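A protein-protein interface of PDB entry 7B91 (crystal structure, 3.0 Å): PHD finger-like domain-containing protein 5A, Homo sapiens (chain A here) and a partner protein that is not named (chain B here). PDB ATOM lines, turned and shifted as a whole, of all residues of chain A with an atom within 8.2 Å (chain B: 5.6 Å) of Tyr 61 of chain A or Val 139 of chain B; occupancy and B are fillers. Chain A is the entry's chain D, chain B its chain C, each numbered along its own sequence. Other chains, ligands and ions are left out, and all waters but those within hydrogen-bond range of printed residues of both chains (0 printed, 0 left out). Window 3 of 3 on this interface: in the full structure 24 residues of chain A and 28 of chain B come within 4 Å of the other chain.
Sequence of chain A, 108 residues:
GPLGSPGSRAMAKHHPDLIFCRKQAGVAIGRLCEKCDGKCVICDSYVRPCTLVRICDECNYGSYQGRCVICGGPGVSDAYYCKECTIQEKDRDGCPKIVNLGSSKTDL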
ATOM      1  N   ALA A  28      38.596   4.312 -30.424  1.00  0.00           N
ATOM      2  CA  ALA A  28      38.554   5.671 -30.948  1.00  0.00           C
ATOM      3  C   ALA A  28      39.950   6.119 -31.361  1.00  0.00           C
ATOM      4  O   ALA A  28      40.913   5.966 -30.602  1.00  0.00           O
ATOM      5  CB  ALA A  28      37.982   6.633 -29.908  1.00  0.00           C
ATOM      6  N   ILE A  55      42.550   6.429 -28.179  1.00  0.00           N
ATOM      7  CA  ILE A  55      42.197   7.116 -26.946  1.00  0.00           C
ATOM      8  C   ILE A  55      41.059   6.366 -26.263  1.00  0.00           C
ATOM      9  O   ILE A  55      40.393   5.515 -26.859  1.00  0.00           O
ATOM     10  CB  ILE A  55      41.809   8.590 -27.185  1.00  0.00           C
ATOM     11  CG1 ILE A  55      40.646   8.688 -28.173  1.00  0.00           C
ATOM     12  CG2 ILE A  55      43.004   9.384 -27.688  1.00  0.00           C
ATOM     13  CD1 ILE A  55      40.161  10.101 -28.388  1.00  0.00           C
ATOM     14  N   CYS A  56      40.844   6.696 -24.992  1.00  0.00           N
ATOM     15  CA  CYS A  56      39.814   6.044 -24.200  1.00  0.00           C
ATOM     16  C   CYS A  56      38.434   6.607 -24.531  1.00  0.00           C
ATOM     17  O   CYS A  56      38.295   7.708 -25.070  1.00  0.00           O
ATOM     18  CB  CYS A  56      40.099   6.208 -22.706  1.00  0.00           C
ATOM     19  SG  CYS A  56      39.682   7.839 -22.058  1.00  0.00           S
ATOM     20  N   ASP A  57      37.401   5.831 -24.185  1.00  0.00           N
ATOM     21  CA  ASP A  57      36.034   6.211 -24.533  1.00  0.00           C
ATOM     22  C   ASP A  57      35.614   7.509 -23.854  1.00  0.00           C
ATOM     23  O   ASP A  57      34.862   8.299 -24.438  1.00  0.00           O
ATOM     24  CB  ASP A  57      35.064   5.087 -24.166  1.00  0.00           C
ATOM     25  CG  ASP A  57      35.085   3.942 -25.164  1.00  0.00           C
ATOM     26  OD1 ASP A  57      35.982   3.925 -26.034  1.00  0.00           O
ATOM     27  OD2 ASP A  57      34.201   3.060 -25.084  1.00  0.00           O
ATOM     28  N   GLU A  58      36.086   7.751 -22.629  1.00  0.00           N
ATOM     29  CA  GLU A  58      35.668   8.947 -21.907  1.00  0.00           C
ATOM     30  C   GLU A  58      36.226  10.208 -22.557  1.00  0.00           C
ATOM     31  O   GLU A  58      35.547  11.241 -22.605  1.00  0.00           O
ATOM     32  CB  GLU A  58      36.100   8.849 -20.442  1.00  0.00           C
ATOM     33  CG  GLU A  58      35.283   9.712 -19.489  1.00  0.00           C
ATOM     34  CD  GLU A  58      35.597   9.431 -18.029  1.00  0.00           C
ATOM     35  OE1 GLU A  58      36.171   8.359 -17.735  1.00  0.00           O
ATOM     36  OE2 GLU A  58      35.270  10.284 -17.175  1.00  0.00           O
ATOM     37  N   CYS A  59      37.453  10.142 -23.078  1.00  0.00           N
ATOM     38  CA  CYS A  59      38.082  11.287 -23.728  1.00  0.00           C
ATOM     39  C   CYS A  59      37.567  11.535 -25.141  1.00  0.00           C
ATOM     40  O   CYS A  59      37.956  12.536 -25.753  1.00  0.00           O
ATOM     41  CB  CYS A  59      39.603  11.106 -23.764  1.00  0.00           C
ATOM     42  SG  CYS A  59      40.435  11.356 -22.177  1.00  0.00           S
ATOM     43  N   ASN A  60      36.710  10.669 -25.674  1.00  0.00           N
ATOM     44  CA  ASN A  60      36.168  10.831 -27.016  1.00  0.00           C
ATOM     45  C   ASN A  60      34.665  11.079 -27.017  1.00  0.00           C
ATOM     46  O   ASN A  60      34.067  11.212 -28.091  1.00  0.00           O
ATOM     47  CB  ASN A  60      36.494   9.595 -27.865  1.00  0.00           C
ATOM     48  CG  ASN A  60      36.292   9.833 -29.353  1.00  0.00           C
ATOM     49  OD1 ASN A  60      36.953  10.680 -29.956  1.00  0.00           O
ATOM     50  ND2 ASN A  60      35.382   9.071 -29.955  1.00  0.00           N
ATOM     51  N   TYR A  61      34.040  11.156 -25.849  1.00  0.00           N
ATOM     52  CA  TYR A  61      32.596  11.277 -25.763  1.00  0.00           C
ATOM     53  C   TYR A  61      32.163  12.735 -25.804  1.00  0.00           C
ATOM     54  O   TYR A  61      32.860  13.626 -25.314  1.00  0.00           O
ATOM     55  CB  TYR A  61      32.076  10.628 -24.482  1.00  0.00           C
ATOM     56  CG  TYR A  61      30.582  10.753 -24.302  1.00  0.00           C
ATOM     57  CD1 TYR A  61      29.714   9.876 -24.941  1.00  0.00           C
ATOM     58  CD2 TYR A  61      30.039  11.742 -23.496  1.00  0.00           C
ATOM     59  CE1 TYR A  61      28.350   9.987 -24.782  1.00  0.00           C
ATOM     60  CE2 TYR A  61      28.678  11.861 -23.332  1.00  0.00           C
ATOM     61  CZ  TYR A  61      27.838  10.980 -23.976  1.00  0.00           C
ATOM     62  OH  TYR A  61      26.480  11.097 -23.813  1.00  0.00           O
ATOM     63  N   GLY A  62      30.987  12.965 -26.381  1.00  0.00           N
ATOM     64  CA  GLY A  62      30.366  14.272 -26.259  1.00  0.00           C
ATOM     65  C   GLY A  62      30.975  15.275 -27.214  1.00  0.00           C
ATOM     66  O   GLY A  62      31.323  14.948 -28.350  1.00  0.00           O
ATOM     67  N   SER A  63      31.096  16.518 -26.748  1.00  0.00           N
ATOM     68  CA  SER A  63      31.730  17.570 -27.528  1.00  0.00           C
ATOM     69  C   SER A  63      33.230  17.359 -27.702  1.00  0.00           C
ATOM     70  O   SER A  63      33.860  18.079 -28.489  1.00  0.00           O
ATOM     71  CB  SER A  63      31.469  18.930 -26.877  1.00  0.00           C
ATOM     72  OG  SER A  63      31.933  18.945 -25.537  1.00  0.00           O
ATOM     73  N   TYR A  64      33.816  16.397 -26.991  1.00  0.00           N
ATOM     74  CA  TYR A  64      35.234  16.091 -27.120  1.00  0.00           C
ATOM     75  C   TYR A  64      35.539  15.212 -28.326  1.00  0.00           C
ATOM     76  O   TYR A  64      36.718  14.974 -28.614  1.00  0.00           O
ATOM     77  CB  TYR A  64      35.741  15.411 -25.845  1.00  0.00           C
ATOM     78  CG  TYR A  64      35.837  16.332 -24.649  1.00  0.00           C
ATOM     79  CD1 TYR A  64      36.036  17.698 -24.812  1.00  0.00           C
ATOM     80  CD2 TYR A  64      35.737  15.835 -23.354  1.00  0.00           C
ATOM     81  CE1 TYR A  64      36.128  18.545 -23.721  1.00  0.00           C
ATOM     82  CE2 TYR A  64      35.828  16.674 -22.256  1.00  0.00           C
ATOM     83  CZ  TYR A  64      36.024  18.028 -22.446  1.00  0.00           C
ATOM     84  OH  TYR A  64      36.116  18.869 -21.360  1.00  0.00           O
ATOM     85  N   GLN A  65      34.516  14.730 -29.029  1.00  0.00           N
ATOM     86  CA  GLN A  65      34.735  13.872 -30.186  1.00  0.00           C
ATOM     87  C   GLN A  65      35.460  14.632 -31.288  1.00  0.00           C
ATOM     88  O   GLN A  65      35.065  15.740 -31.663  1.00  0.00           O
ATOM     89  CB  GLN A  65      33.398  13.331 -30.698  1.00  0.00           C
ATOM     90  CG  GLN A  65      33.307  13.146 -32.211  1.00  0.00           C
ATOM     91  CD  GLN A  65      34.021  11.900 -32.720  1.00  0.00           C
ATOM     92  OE1 GLN A  65      35.067  11.505 -32.203  1.00  0.00           O
ATOM     93  NE2 GLN A  65      33.449  11.275 -33.742  1.00  0.00           N
ATOM     94  N   GLY A  66      36.534  14.035 -31.798  1.00  0.00           N
ATOM     95  CA  GLY A  66      37.263  14.618 -32.906  1.00  0.00           C
ATOM     96  C   GLY A  66      38.148  15.791 -32.558  1.00  0.00           C
ATOM     97  O   GLY A  66      38.746  16.382 -33.461  1.00  0.00           O
ATOM     98  N   LYS A 105      35.253  21.481 -16.740  1.00  0.00           N
ATOM     99  CA  LYS A 105      34.838  21.080 -18.079  1.00  0.00           C
ATOM    100  C   LYS A 105      34.039  22.158 -18.800  1.00  0.00           C
ATOM    101  O   LYS A 105      33.528  21.899 -19.894  1.00  0.00           O
ATOM    102  CB  LYS A 105      34.030  19.778 -18.015  1.00  0.00           C
ATOM    103  CG  LYS A 105      34.852  18.590 -17.534  1.00  0.00           C
ATOM    104  CD  LYS A 105      34.079  17.278 -17.548  1.00  0.00           C
ATOM    105  CE  LYS A 105      34.127  16.612 -18.914  1.00  0.00           C
ATOM    106  NZ  LYS A 105      32.906  16.863 -19.724  1.00  0.00           N
ATOM    107  N   HIS B  98      26.494  15.616 -19.107  1.00  0.00           N
ATOM    108  CA  HIS B  98      27.153  14.313 -19.035  1.00  0.00           C
ATOM    109  C   HIS B  98      27.595  13.998 -17.610  1.00  0.00           C
ATOM    110  O   HIS B  98      27.442  12.861 -17.141  1.00  0.00           O
ATOM    111  CB  HIS B  98      28.348  14.265 -19.990  1.00  0.00           C
ATOM    112  CG  HIS B  98      29.126  12.986 -19.921  1.00  0.00           C
ATOM    113  ND1 HIS B  98      28.553  11.752 -20.148  1.00  0.00           N
ATOM    114  CD2 HIS B  98      30.431  12.748 -19.648  1.00  0.00           C
ATOM    115  CE1 HIS B  98      29.472  10.811 -20.020  1.00  0.00           C
ATOM    116  NE2 HIS B  98      30.619  11.389 -19.716  1.00  0.00           N
ATOM    117  N   ASP B 134      19.711  16.701 -30.086  1.00  0.00           N
ATOM    118  CA  ASP B 134      21.090  16.317 -29.818  1.00  0.00           C
ATOM    119  C   ASP B 134      21.195  14.803 -29.671  1.00  0.00           C
ATOM    120  O   ASP B 134      20.487  14.197 -28.861  1.00  0.00           O
ATOM    121  CB  ASP B 134      21.597  17.013 -28.555  1.00  0.00           C
ATOM    122  CG  ASP B 134      23.109  16.961 -28.423  1.00  0.00           C
ATOM    123  OD1 ASP B 134      23.777  16.493 -29.370  1.00  0.00           O
ATOM    124  OD2 ASP B 134      23.631  17.387 -27.370  1.00  0.00           O
ATOM    125  N   TYR B 135      22.083  14.195 -30.461  1.00  0.00           N
ATOM    126  CA  TYR B 135      22.265  12.747 -30.413  1.00  0.00           C
ATOM    127  C   TYR B 135      22.776  12.297 -29.046  1.00  0.00           C
ATOM    128  O   TYR B 135      22.340  11.266 -28.513  1.00  0.00           O
ATOM    129  CB  TYR B 135      23.219  12.328 -31.535  1.00  0.00           C
ATOM    130  CG  TYR B 135      23.894  10.983 -31.368  1.00  0.00           C
ATOM    131  CD1 TYR B 135      23.291   9.818 -31.822  1.00  0.00           C
ATOM    132  CD2 TYR B 135      25.149  10.886 -30.780  1.00  0.00           C
ATOM    133  CE1 TYR B 135      23.914   8.591 -31.680  1.00  0.00           C
ATOM    134  CE2 TYR B 135      25.776   9.667 -30.630  1.00  0.00           C
ATOM    135  CZ  TYR B 135      25.157   8.522 -31.082  1.00  0.00           C
ATOM    136  OH  TYR B 135      25.788   7.308 -30.933  1.00  0.00           O
ATOM    137  N   TYR B 136      23.689  13.072 -28.454  1.00  0.00           N
ATOM    138  CA  TYR B 136      24.223  12.716 -27.145  1.00  0.00           C
ATOM    139  C   TYR B 136      23.168  12.843 -26.053  1.00  0.00           C
ATOM    140  O   TYR B 136      23.169  12.054 -25.100  1.00  0.00           O
ATOM    141  CB  TYR B 136      25.443  13.581 -26.832  1.00  0.00           C
ATOM    142  CG  TYR B 136      26.612  13.304 -27.753  1.00  0.00           C
ATOM    143  CD1 TYR B 136      26.982  12.000 -28.060  1.00  0.00           C
ATOM    144  CD2 TYR B 136      27.333  14.341 -28.328  1.00  0.00           C
ATOM    145  CE1 TYR B 136      28.045  11.736 -28.906  1.00  0.00           C
ATOM    146  CE2 TYR B 136      28.398  14.088 -29.176  1.00  0.00           C
ATOM    147  CZ  TYR B 136      28.750  12.785 -29.460  1.00  0.00           C
ATOM    148  OH  TYR B 136      29.809  12.532 -30.302  1.00  0.00           O
ATOM    149  N   ALA B 137      22.254  13.809 -26.177  1.00  0.00           N
ATOM    150  CA  ALA B 137      21.141  13.886 -25.237  1.00  0.00           C
ATOM    151  C   ALA B 137      20.278  12.632 -25.310  1.00  0.00           C
ATOM    152  O   ALA B 137      19.828  12.116 -24.281  1.00  0.00           O
ATOM    153  CB  ALA B 137      20.303  15.135 -25.512  1.00  0.00           C
ATOM    154  N   ARG B 138      20.056  12.116 -26.522  1.00  0.00           N
ATOM    155  CA  ARG B 138      19.286  10.887 -26.669  1.00  0.00           C
ATOM    156  C   ARG B 138      20.008   9.701 -26.042  1.00  0.00           C
ATOM    157  O   ARG B 138      19.387   8.891 -25.339  1.00  0.00           O
ATOM    158  CB  ARG B 138      18.997  10.618 -28.148  1.00  0.00           C
ATOM    159  CG  ARG B 138      18.101  11.657 -28.808  1.00  0.00           C
ATOM    160  CD  ARG B 138      17.566  11.165 -30.146  1.00  0.00           C
ATOM    161  NE  ARG B 138      18.635  10.887 -31.102  1.00  0.00           N
ATOM    162  CZ  ARG B 138      19.121  11.777 -31.962  1.00  0.00           C
ATOM    163  NH1 ARG B 138      20.095  11.433 -32.793  1.00  0.00           N
ATOM    164  NH2 ARG B 138      18.632  13.011 -31.993  1.00  0.00           N
ATOM    165  N   VAL B 139      21.317   9.574 -26.281  1.00  0.00           N
ATOM    166  CA  VAL B 139      22.019   8.430 -25.701  1.00  0.00           C
ATOM    167  C   VAL B 139      22.062   8.545 -24.180  1.00  0.00           C
ATOM    168  O   VAL B 139      21.975   7.531 -23.475  1.00  0.00           O
ATOM    169  CB  VAL B 139      23.429   8.257 -26.310  1.00  0.00           C
ATOM    170  CG1 VAL B 139      23.366   8.301 -27.831  1.00  0.00           C
ATOM    171  CG2 VAL B 139      24.418   9.277 -25.770  1.00  0.00           C
ATOM    172  N   GLU B 140      22.140   9.765 -23.643  1.00  0.00           N
ATOM    173  CA  GLU B 140      22.136   9.928 -22.192  1.00  0.00           C
ATOM    174  C   GLU B 140      20.768   9.598 -21.600  1.00  0.00           C
ATOM    175  O   GLU B 140      20.682   8.965 -20.540  1.00  0.00           O
ATOM    176  CB  GLU B 140      22.567  11.348 -21.827  1.00  0.00           C
ATOM    177  CG  GLU B 140      24.078  11.540 -21.830  1.00  0.00           C
ATOM    178  CD  GLU B 140      24.495  12.956 -22.184  1.00  0.00           C
ATOM    179  OE1 GLU B 140      23.663  13.701 -22.743  1.00  0.00           O
ATOM    180  OE2 GLU B 140      25.654  13.327 -21.903  1.00  0.00           O
ATOM    181  N   GLY B 141      19.689  10.010 -22.269  1.00  0.00           N
ATOM    182  CA  GLY B 141      18.363   9.618 -21.816  1.00  0.00           C
ATOM    183  C   GLY B 141      18.170   8.113 -21.818  1.00  0.00           C
ATOM    184  O   GLY B 141      17.608   7.545 -20.875  1.00  0.00           O
ATOM    185  N   ARG B 142      18.641   7.444 -22.875  1.00  0.00           N
ATOM    186  CA  ARG B 142      18.540   5.989 -22.924  1.00  0.00           C
ATOM    187  C   ARG B 142      19.369   5.339 -21.821  1.00  0.00           C
ATOM    188  O   ARG B 142      18.930   4.365 -21.195  1.00  0.00           O
ATOM    189  CB  ARG B 142      18.963   5.475 -24.302  1.00  0.00           C
ATOM    190  CG  ARG B 142      18.019   5.888 -25.422  1.00  0.00           C
ATOM    191  CD  ARG B 142      18.231   5.060 -26.680  1.00  0.00           C
ATOM    192  NE  ARG B 142      19.505   5.352 -27.333  1.00  0.00           N
ATOM    193  CZ  ARG B 142      19.654   6.237 -28.316  1.00  0.00           C
ATOM    194  NH1 ARG B 142      18.607   6.920 -28.759  1.00  0.00           N
ATOM    195  NH2 ARG B 142      20.848   6.439 -28.854  1.00  0.00           N
ATOM    196  N   GLU B 143      20.569   5.869 -21.563  1.00  0.00           N
ATOM    197  CA  GLU B 143      21.394   5.350 -20.476  1.00  0.00           C
ATOM    198  C   GLU B 143      20.689   5.496 -19.134  1.00  0.00           C
ATOM    199  O   GLU B 143      20.715   4.577 -18.306  1.00  0.00           O
ATOM    200  CB  GLU B 143      22.745   6.069 -20.460  1.00  0.00           C
ATOM    201  CG  GLU B 143      23.624   5.736 -19.263  1.00  0.00           C
ATOM    202  CD  GLU B 143      25.032   6.295 -19.392  1.00  0.00           C
ATOM    203  OE1 GLU B 143      25.415   6.691 -20.514  1.00  0.00           O
ATOM    204  OE2 GLU B 143      25.753   6.341 -18.373  1.00  0.00           O
ATOM    205  N   ILE B 144      20.044   6.642 -18.906  1.00  0.00           N
ATOM    206  CA  ILE B 144      19.344   6.862 -17.642  1.00  0.00           C
ATOM    207  C   ILE B 144      18.174   5.896 -17.496  1.00  0.00           C
ATOM    208  O   ILE B 144      17.967   5.313 -16.425  1.00  0.00           O
ATOM    209  CB  ILE B 144      18.891   8.329 -17.525  1.00  0.00           C
ATOM    210  CG1 ILE B 144      20.101   9.248 -17.354  1.00  0.00           C
ATOM    211  CG2 ILE B 144      17.918   8.500 -16.366  1.00  0.00           C
ATOM    212  CD1 ILE B 144      19.739  10.685 -17.048  1.00  0.00           C
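O of Gly 62 of chain A lies close to OH of Tyr 136 of chain B (3.5 Å).
The side-chain carboxylate (OE2) of Glu 140 of chain B sits at hydrogen-bond distance from the side-chain hydroxyl (OH) of Tyr 61 of chain A (3.1 Å).
OD1 of Asn 60 of chain A lies close to OE1 of Gln 65 of chain A (3.0 Å).
Tyr 61 of chain A touches His 98 of chain B (CE2 to ND1, 3.2 Å).
OH of Tyr 61 of chain A touches O of Tyr 136 of chain B, 3.7 Å away.
CG2 of Val 139 of chain B touches OH of Tyr 61 of chain A, 3.4 Å away.
Gln 65 of chain A touches Tyr 136 of chain B (CB to OH, 3.7 Å).
Of the printed residues of chain B, Tyr 61 of chain A touches His 98 (3.2 Å), Tyr 136 (3.7 Å), Val 139 (3.4 Å) and Glu 140 (3.1 Å).
Printed residues of chain B within 4 Å of Gly 62 of chain A: Tyr 136 (3.2 Å).
Tyr 64 of chain A touches none of the printed residues of chain B.
Of the printed residues of chain B, Gln 65 of chain A touches Tyr 136 (3.7 Å).
Of the printed residues of chain A, His 98 of chain B touches Tyr 61.
Asp 134 of chain B touches none of the printed residues of chain A.
Of the printed residues of chain A, Tyr 136 of chain B touches Tyr 61 (3.7 Å), Gly 62 (3.2 Å) and Gln 65 (3.7 Å).
Of the printed residues of chain A, Val 139 of chain B touches Tyr 61 (3.4 Å).
The nearest residue of chain A that does not touch Val 139 of chain B is Gly 62 of chain A (7.6 Å).
Of the 12 printed residues of chain B, 4 touch a printed residue of chain A.
Hydrophobic or aromatic side chains of chain B that line the printed part of chain A: His 98, Tyr 136 and Val 139.
Of the 14 printed residues of chain A, 3 touch a printed residue of chain B.
Among the printed residues, 6 pairs touch across the chains.
Among the printed residues, no Asp or Glu carboxylate lies within 4 Å of a Lys or Arg side-chain nitrogen of the other chain.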
